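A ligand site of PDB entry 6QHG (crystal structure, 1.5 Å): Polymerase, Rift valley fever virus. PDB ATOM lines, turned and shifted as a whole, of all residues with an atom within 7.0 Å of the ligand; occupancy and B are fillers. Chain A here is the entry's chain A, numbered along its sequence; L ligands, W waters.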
ATOM      1  N   GLY A   8      29.947 -11.863 -15.701  1.00  0.00           N
ATOM      2  CA  GLY A   8      30.667 -11.813 -14.446  1.00  0.00           C
ATOM      3  C   GLY A   8      30.477 -13.115 -13.691  1.00  0.00           C
ATOM      4  O   GLY A   8      30.037 -14.109 -14.261  1.00  0.00           O
ATOM      5  N   GLY A   9      30.814 -13.078 -12.414  1.00  0.00           N
ATOM      6  CA  GLY A   9      30.647 -14.267 -11.595  1.00  0.00           C
ATOM      7  C   GLY A   9      31.035 -13.961 -10.163  1.00  0.00           C
ATOM      8  O   GLY A   9      31.530 -12.887  -9.849  1.00  0.00           O
ATOM      9  N   PHE A  10      30.776 -14.933  -9.305  1.00  0.00           N
ATOM     10  CA  PHE A  10      31.137 -14.767  -7.900  1.00  0.00           C
ATOM     11  C   PHE A  10      32.641 -14.909  -7.726  1.00  0.00           C
ATOM     12  O   PHE A  10      33.242 -15.904  -8.163  1.00  0.00           O
ATOM     13  CB  PHE A  10      30.396 -15.778  -7.037  1.00  0.00           C
ATOM     14  CG  PHE A  10      28.953 -15.439  -6.834  1.00  0.00           C
ATOM     15  CD1 PHE A  10      28.569 -14.553  -5.846  1.00  0.00           C
ATOM     16  CD2 PHE A  10      27.972 -15.990  -7.665  1.00  0.00           C
ATOM     17  CE1 PHE A  10      27.237 -14.221  -5.658  1.00  0.00           C
ATOM     18  CE2 PHE A  10      26.627 -15.658  -7.495  1.00  0.00           C
ATOM     19  CZ  PHE A  10      26.263 -14.776  -6.494  1.00  0.00           C
ATOM     20  N   LYS A  12      33.701 -14.213  -4.440  1.00  0.00           N
ATOM     21  CA  LYS A  12      33.547 -14.806  -3.121  1.00  0.00           C
ATOM     22  C   LYS A  12      32.217 -15.548  -3.135  1.00  0.00           C
ATOM     23  O   LYS A  12      31.146 -14.936  -3.140  1.00  0.00           O
ATOM     24  CB  LYS A  12      33.579 -13.759  -2.012  1.00  0.00           C
ATOM     25  CG  LYS A  12      33.411 -14.329  -0.595  1.00  0.00           C
ATOM     26  CD  LYS A  12      33.423 -13.235   0.461  1.00  0.00           C
ATOM     27  CE  LYS A  12      33.056 -13.775   1.844  1.00  0.00           C
ATOM     28  NZ  LYS A  12      33.917 -14.923   2.260  1.00  0.00           N
ATOM     29  N   ARG A  13      32.290 -16.874  -3.174  1.00  0.00           N
ATOM     30  CA  ARG A  13      31.099 -17.688  -3.159  1.00  0.00           C
ATOM     31  C   ARG A  13      30.488 -17.665  -1.769  1.00  0.00           C
ATOM     32  O   ARG A  13      31.194 -17.621  -0.767  1.00  0.00           O
ATOM     33  CB  ARG A  13      31.462 -19.128  -3.530  1.00  0.00           C
ATOM     34  CG  ARG A  13      32.294 -19.221  -4.797  1.00  0.00           C
ATOM     35  CD  ARG A  13      33.068 -20.521  -4.855  1.00  0.00           C
ATOM     36  NE  ARG A  13      32.185 -21.685  -4.921  1.00  0.00           N
ATOM     37  CZ  ARG A  13      31.743 -22.215  -6.056  1.00  0.00           C
ATOM     38  NH1 ARG A  13      32.087 -21.685  -7.224  1.00  0.00           N
ATOM     39  NH2 ARG A  13      30.940 -23.275  -6.028  1.00  0.00           N
ATOM     40  N   GLN A  14      29.158 -17.682  -1.722  1.00  0.00           N
ATOM     41  CA  GLN A  14      28.485 -17.900  -0.447  1.00  0.00           C
ATOM     42  C   GLN A  14      28.799 -19.300   0.048  1.00  0.00           C
ATOM     43  O   GLN A  14      29.155 -20.207  -0.704  1.00  0.00           O
ATOM     44  CB  GLN A  14      26.973 -17.741  -0.609  1.00  0.00           C
ATOM     45  CG  GLN A  14      26.521 -16.294  -0.747  1.00  0.00           C
ATOM     46  CD  GLN A  14      25.013 -16.164  -0.796  1.00  0.00           C
ATOM     47  OE1 GLN A  14      24.369 -16.602  -1.750  1.00  0.00           O
ATOM     48  NE2 GLN A  14      24.443 -15.600   0.255  1.00  0.00           N
ATOM     49  N   GLN A  15      28.651 -19.480   1.359  1.00  0.00           N
ATOM     50  CA  GLN A  15      28.690 -20.829   1.907  1.00  0.00           C
ATOM     51  C   GLN A  15      27.452 -21.584   1.442  1.00  0.00           C
ATOM     52  O   GLN A  15      26.447 -20.996   1.037  1.00  0.00           O
ATOM     53  CB  GLN A  15      28.732 -20.764   3.433  1.00  0.00           C
ATOM     54  CG  GLN A  15      29.919 -19.978   3.956  1.00  0.00           C
ATOM     55  CD  GLN A  15      29.756 -19.558   5.407  1.00  0.00           C
ATOM     56  OE1 GLN A  15      29.524 -18.384   5.701  1.00  0.00           O
ATOM     57  NE2 GLN A  15      29.876 -20.511   6.328  1.00  0.00           N
ATOM     58  N   SER A  16      27.525 -22.918   1.469  1.00  0.00           N
ATOM     59  CA  SER A  16      26.407 -23.695   0.957  1.00  0.00           C
ATOM     60  C   SER A  16      26.332 -25.039   1.658  1.00  0.00           C
ATOM     61  O   SER A  16      27.321 -25.544   2.199  1.00  0.00           O
ATOM     62  CB  SER A  16      26.501 -23.914  -0.565  1.00  0.00           C
ATOM     63  OG  SER A  16      27.566 -24.796  -0.885  1.00  0.00           O
ATOM     64  N   VAL A  23      20.722 -27.419  -3.103  1.00  0.00           N
ATOM     65  CA  VAL A  23      21.774 -26.585  -2.540  1.00  0.00           C
ATOM     66  C   VAL A  23      21.135 -25.329  -1.950  1.00  0.00           C
ATOM     67  O   VAL A  23      20.245 -24.715  -2.553  1.00  0.00           O
ATOM     68  CB  VAL A  23      22.843 -26.268  -3.584  1.00  0.00           C
ATOM     69  CG1 VAL A  23      22.265 -25.468  -4.734  1.00  0.00           C
ATOM     70  CG2 VAL A  23      24.018 -25.527  -2.936  1.00  0.00           C
ATOM     71  N   TYR A  25      22.297 -21.613  -0.193  1.00  0.00           N
ATOM     72  CA  TYR A  25      23.398 -20.677  -0.036  1.00  0.00           C
ATOM     73  C   TYR A  25      23.149 -19.768   1.163  1.00  0.00           C
ATOM     74  O   TYR A  25      22.012 -19.439   1.492  1.00  0.00           O
ATOM     75  CB  TYR A  25      23.564 -19.835  -1.297  1.00  0.00           C
ATOM     76  CG  TYR A  25      24.031 -20.617  -2.506  1.00  0.00           C
ATOM     77  CD1 TYR A  25      25.372 -20.990  -2.623  1.00  0.00           C
ATOM     78  CD2 TYR A  25      23.157 -20.960  -3.523  1.00  0.00           C
ATOM     79  CE1 TYR A  25      25.813 -21.690  -3.728  1.00  0.00           C
ATOM     80  CE2 TYR A  25      23.599 -21.673  -4.633  1.00  0.00           C
ATOM     81  CZ  TYR A  25      24.922 -22.035  -4.727  1.00  0.00           C
ATOM     82  OH  TYR A  25      25.366 -22.739  -5.823  1.00  0.00           O
ATOM     83  N   TYR A  26      24.245 -19.358   1.815  1.00  0.00           N
ATOM     84  CA  TYR A  26      24.129 -18.484   2.979  1.00  0.00           C
ATOM     85  C   TYR A  26      25.470 -17.787   3.191  1.00  0.00           C
ATOM     86  O   TYR A  26      26.478 -18.120   2.563  1.00  0.00           O
ATOM     87  CB  TYR A  26      23.676 -19.245   4.231  1.00  0.00           C
ATOM     88  CG  TYR A  26      24.638 -20.304   4.726  1.00  0.00           C
ATOM     89  CD1 TYR A  26      24.675 -21.571   4.145  1.00  0.00           C
ATOM     90  CD2 TYR A  26      25.488 -20.050   5.795  1.00  0.00           C
ATOM     91  CE1 TYR A  26      25.547 -22.545   4.609  1.00  0.00           C
ATOM     92  CE2 TYR A  26      26.366 -21.016   6.260  1.00  0.00           C
ATOM     93  CZ  TYR A  26      26.388 -22.259   5.672  1.00  0.00           C
ATOM     94  OH  TYR A  26      27.269 -23.216   6.153  1.00  0.00           O
ATOM     95  N   VAL A  28      27.985 -14.427   3.026  1.00  0.00           N
ATOM     96  CA  VAL A  28      28.277 -13.289   2.157  1.00  0.00           C
ATOM     97  C   VAL A  28      28.760 -13.786   0.798  1.00  0.00           C
ATOM     98  O   VAL A  28      29.608 -14.686   0.722  1.00  0.00           O
ATOM     99  CB  VAL A  28      29.323 -12.345   2.784  1.00  0.00           C
ATOM    100  CG1 VAL A  28      29.745 -11.254   1.807  1.00  0.00           C
ATOM    101  CG2 VAL A  28      28.785 -11.734   4.075  1.00  0.00           C
ATOM    102  N   GLY A  29      28.209 -13.220  -0.267  1.00  0.00           N
ATOM    103  CA  GLY A  29      28.703 -13.450  -1.607  1.00  0.00           C
ATOM    104  C   GLY A  29      29.105 -12.145  -2.262  1.00  0.00           C
ATOM    105  O   GLY A  29      28.484 -11.109  -2.032  1.00  0.00           O
ATOM    106  N   ILE A  30      30.157 -12.198  -3.076  1.00  0.00           N
ATOM    107  CA  ILE A  30      30.605 -11.029  -3.832  1.00  0.00           C
ATOM    108  C   ILE A  30      30.666 -11.419  -5.298  1.00  0.00           C
ATOM    109  O   ILE A  30      31.401 -12.347  -5.667  1.00  0.00           O
ATOM    110  CB  ILE A  30      31.968 -10.494  -3.374  1.00  0.00           C
ATOM    111  CG1 ILE A  30      31.943 -10.133  -1.889  1.00  0.00           C
ATOM    112  CG2 ILE A  30      32.338  -9.290  -4.235  1.00  0.00           C
ATOM    113  CD1 ILE A  30      33.294  -9.752  -1.342  1.00  0.00           C
ATOM    114  N   TRP A  31      29.919 -10.708  -6.127  1.00  0.00           N
ATOM    115  CA  TRP A  31      29.870 -10.919  -7.563  1.00  0.00           C
ATOM    116  C   TRP A  31      30.556  -9.728  -8.220  1.00  0.00           C
ATOM    117  O   TRP A  31      30.328  -8.581  -7.834  1.00  0.00           O
ATOM    118  CB  TRP A  31      28.407 -11.013  -8.008  1.00  0.00           C
ATOM    119  CG  TRP A  31      28.178 -11.297  -9.472  1.00  0.00           C
ATOM    120  CD1 TRP A  31      27.869 -12.506 -10.027  1.00  0.00           C
ATOM    121  CD2 TRP A  31      28.175 -10.349 -10.560  1.00  0.00           C
ATOM    122  NE1 TRP A  31      27.700 -12.369 -11.390  1.00  0.00           N
ATOM    123  CE2 TRP A  31      27.876 -11.057 -11.738  1.00  0.00           C
ATOM    124  CE3 TRP A  31      28.401  -8.969 -10.643  1.00  0.00           C
ATOM    125  CZ2 TRP A  31      27.802 -10.439 -12.988  1.00  0.00           C
ATOM    126  CZ3 TRP A  31      28.327  -8.351 -11.893  1.00  0.00           C
ATOM    127  CH2 TRP A  31      28.037  -9.096 -13.044  1.00  0.00           C
ATOM    128  N   ILE A  44      25.951  -9.701  -1.744  1.00  0.00           N
ATOM    129  CA  ILE A  44      24.698 -10.241  -1.223  1.00  0.00           C
ATOM    130  C   ILE A  44      24.969 -10.956   0.102  1.00  0.00           C
ATOM    131  O   ILE A  44      26.081 -11.394   0.376  1.00  0.00           O
ATOM    132  CB  ILE A  44      23.996 -11.171  -2.229  1.00  0.00           C
ATOM    133  CG1 ILE A  44      24.879 -12.395  -2.542  1.00  0.00           C
ATOM    134  CG2 ILE A  44      23.670 -10.396  -3.493  1.00  0.00           C
ATOM    135  CD1 ILE A  44      24.217 -13.428  -3.470  1.00  0.00           C
ATOM    136  N   ASN A  46      22.727 -13.467   3.277  1.00  0.00           N
ATOM    137  CA  ASN A  46      21.524 -13.986   3.926  1.00  0.00           C
ATOM    138  C   ASN A  46      21.908 -15.072   4.914  1.00  0.00           C
ATOM    139  O   ASN A  46      22.942 -15.738   4.760  1.00  0.00           O
ATOM    140  CB  ASN A  46      20.521 -14.547   2.914  1.00  0.00           C
ATOM    141  CG  ASN A  46      21.093 -15.669   2.061  1.00  0.00           C
ATOM    142  OD1 ASN A  46      21.704 -15.411   1.038  1.00  0.00           O
ATOM    143  ND2 ASN A  46      20.858 -16.917   2.462  1.00  0.00           N
ATOM    144  N   PRO A  52      18.616 -14.130  -0.612  1.00  0.00           N
ATOM    145  CA  PRO A  52      19.772 -13.220  -0.570  1.00  0.00           C
ATOM    146  C   PRO A  52      19.341 -11.773  -0.740  1.00  0.00           C
ATOM    147  O   PRO A  52      18.449 -11.462  -1.533  1.00  0.00           O
ATOM    148  CB  PRO A  52      20.637 -13.690  -1.748  1.00  0.00           C
ATOM    149  CG  PRO A  52      19.696 -14.465  -2.646  1.00  0.00           C
ATOM    150  CD  PRO A  52      18.691 -15.093  -1.729  1.00  0.00           C
ATOM    151  N   ASP A  78      17.321 -12.805 -11.858  1.00  0.00           N
ATOM    152  CA  ASP A  78      17.905 -14.106 -12.166  1.00  0.00           C
ATOM    153  C   ASP A  78      18.367 -14.819 -10.906  1.00  0.00           C
ATOM    154  O   ASP A  78      18.197 -16.033 -10.762  1.00  0.00           O
ATOM    155  CB  ASP A  78      19.092 -13.941 -13.115  1.00  0.00           C
ATOM    156  CG  ASP A  78      18.729 -13.354 -14.470  1.00  0.00           C
ATOM    157  OD1 ASP A  78      19.662 -12.995 -15.230  1.00  0.00           O
ATOM    158  OD2 ASP A  78      17.529 -13.259 -14.800  1.00  0.00           O
ATOM    159  N   MET A  79      18.976 -14.073  -9.978  1.00  0.00           N
ATOM    160  CA  MET A  79      19.568 -14.653  -8.760  1.00  0.00           C
ATOM    161  C   MET A  79      18.621 -14.816  -7.570  1.00  0.00           C
ATOM    162  O   MET A  79      19.028 -15.381  -6.550  1.00  0.00           O
ATOM    163  CB  MET A  79      20.762 -13.813  -8.299  1.00  0.00           C
ATOM    164  CG  MET A  79      21.891 -13.787  -9.297  1.00  0.00           C
ATOM    165  SD  MET A  79      22.920 -15.436  -9.134  1.00  0.00           S
ATOM    166  CE  MET A  79      22.930 -15.624  -7.215  1.00  0.00           C
ATOM    167  N   VAL A  81      17.621 -12.314  -5.787  1.00  0.00           N
ATOM    168  CA  VAL A  81      18.138 -11.352  -4.819  1.00  0.00           C
ATOM    169  C   VAL A  81      17.113 -10.245  -4.616  1.00  0.00           C
ATOM    170  O   VAL A  81      16.582  -9.695  -5.580  1.00  0.00           O
ATOM    171  CB  VAL A  81      19.477 -10.781  -5.304  1.00  0.00           C
ATOM    172  CG1 VAL A  81      19.898  -9.567  -4.455  1.00  0.00           C
ATOM    173  CG2 VAL A  81      20.553 -11.864  -5.297  1.00  0.00           C
HETATM  174  P1  LIG L   1      30.836 -25.536  -9.575  1.00  0.00           P
HETATM  175  O1  LIG L   1      30.123 -26.818  -9.226  1.00  0.00           O
HETATM  176  O2  LIG L   1      31.801 -25.811 -10.696  1.00  0.00           O
HETATM  177  O3  LIG L   1      31.577 -24.989  -8.368  1.00  0.00           O
HETATM  178  O4  LIG L   1      29.762 -24.491 -10.077  1.00  0.00           O
HETATM  179  P2  LIG L   1      29.685 -22.923  -9.838  1.00  0.00           P
HETATM  180  O5  LIG L   1      28.831 -22.629  -8.636  1.00  0.00           O
HETATM  181  O6  LIG L   1      31.075 -22.338  -9.648  1.00  0.00           O
HETATM  182  O7  LIG L   1      29.026 -22.368 -11.167  1.00  0.00           O
HETATM  183  P3  LIG L   1      28.654 -20.869 -11.501  1.00  0.00           P
HETATM  184  O8  LIG L   1      29.667 -19.936 -10.890  1.00  0.00           O
HETATM  185  O9  LIG L   1      28.607 -20.681 -12.997  1.00  0.00           O
HETATM  186  O10 LIG L   1      27.246 -20.507 -10.895  1.00  0.00           O
HETATM  187  C1  LIG L   1      26.073 -20.823 -11.626  1.00  0.00           C
HETATM  188  C2  LIG L   1      24.887 -20.308 -10.869  1.00  0.00           C
HETATM  189  O11 LIG L   1      24.757 -21.047  -9.437  1.00  0.00           O
HETATM  190  C3  LIG L   1      25.030 -19.055 -10.554  1.00  0.00           C
HETATM  191  O12 LIG L   1      24.667 -18.156 -11.691  1.00  0.00           O
HETATM  192  C4  LIG L   1      24.009 -18.915  -9.422  1.00  0.00           C
HETATM  193  O13 LIG L   1      22.750 -19.047  -9.898  1.00  0.00           O
HETATM  194  C5  LIG L   1      24.330 -20.150  -8.579  1.00  0.00           C
HETATM  195  N1  LIG L   1      25.387 -19.807  -7.660  1.00  0.00           N
HETATM  196  C6  LIG L   1      26.808 -20.197  -7.725  1.00  0.00           C
HETATM  197  N2  LIG L   1      27.465 -19.610  -6.536  1.00  0.00           N
HETATM  198  C7  LIG L   1      28.838 -19.736  -6.208  1.00  0.00           C
HETATM  199  C8  LIG L   1      26.453 -18.919  -5.820  1.00  0.00           C
HETATM  200  C9  LIG L   1      26.490 -18.137  -4.548  1.00  0.00           C
HETATM  201  O14 LIG L   1      27.521 -17.991  -3.915  1.00  0.00           O
HETATM  202  N3  LIG L   1      25.303 -17.549  -4.062  1.00  0.00           N
HETATM  203  C10 LIG L   1      24.069 -17.696  -4.764  1.00  0.00           C
HETATM  204  N4  LIG L   1      22.894 -17.095  -4.254  1.00  0.00           N
HETATM  205  N5  LIG L   1      24.022 -18.451  -5.996  1.00  0.00           N
HETATM  206  C11 LIG L   1      25.224 -19.049  -6.493  1.00  0.00           C
HETATM  207  O   HOH W   1      29.408 -17.242 -10.875  1.00  0.00           O
HETATM  208  O   HOH W   2      21.533 -16.996  -1.264  1.00  0.00           O
HETATM  209  O   HOH W   3      26.942 -16.098 -11.488  1.00  0.00           O
HETATM  210  O   HOH W   4      27.466 -26.199  -8.242  1.00  0.00           O
HETATM  211  O   HOH W   5      20.436 -17.383  -5.473  1.00  0.00           O
HETATM  212  O   HOH W   6      21.566 -21.904 -10.640  1.00  0.00           O
HETATM  213  O   HOH W   7      27.687 -19.084 -14.602  1.00  0.00           O
HETATM  214  O   HOH W   8      20.832 -18.837  -7.926  1.00  0.00           O
HETATM  215  O   HOH W   9      34.253 -24.181  -8.980  1.00  0.00           O
HETATM  216  O   HOH W  10      26.266 -23.879  -9.685  1.00  0.00           O
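NE2 of Gln 14 is in hydrogen-bond range of OD1 of Asn 46 (2.9 Å). O of Tyr 25 is in hydrogen-bond range of ND2 of Asn 46, at 2.9 Å. The backbone carbonyl oxygen of Ile 44 lies within hydrogen-bond range of the backbone NH of Gly 29 (2.9 Å).
Merely in contact with the ligand: Phe 10 (3.7 Å) and Ile 44 (3.98 Å). Hydrophobic or aromatic side chains that line the ligand: Phe 10, Tyr 25, Ile 44 and Met 79. Of the 21 residues printed, 6 come within 4 Å of the ligand.
Water W1 bridges O8 of the ligand (2.7 Å) and N of Phe 10 (3.1 Å). Water W5 bridges O of Met 79 and N4 of the ligand. Water W2 lies within hydrogen-bond range of the side-chain amide oxygen (OD1) of Asn 46 (2.8 Å), the side-chain amide oxygen (OE1) of Gln 14 (2.9 Å) and a nitrogen (N4) of the ligand (3.3 Å).
O14 of the ligand is in hydrogen-bond range of N of Gln 14 (2.8 Å). The side-chain amide oxygen of Gln 14 lies within hydrogen-bond range of a nitrogen (N3) of the ligand (2.7 Å). NH1 of Arg 13 is in salt-bridge range of O6 of the ligand (2.7 Å). The side-chain sulfur (SD) of Met 79 lies close to an oxygen (O13) of the ligand (3.7 Å). The side-chain hydroxyl (OH) of Tyr 25 sits close to a nitrogen (N1) of the ligand.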
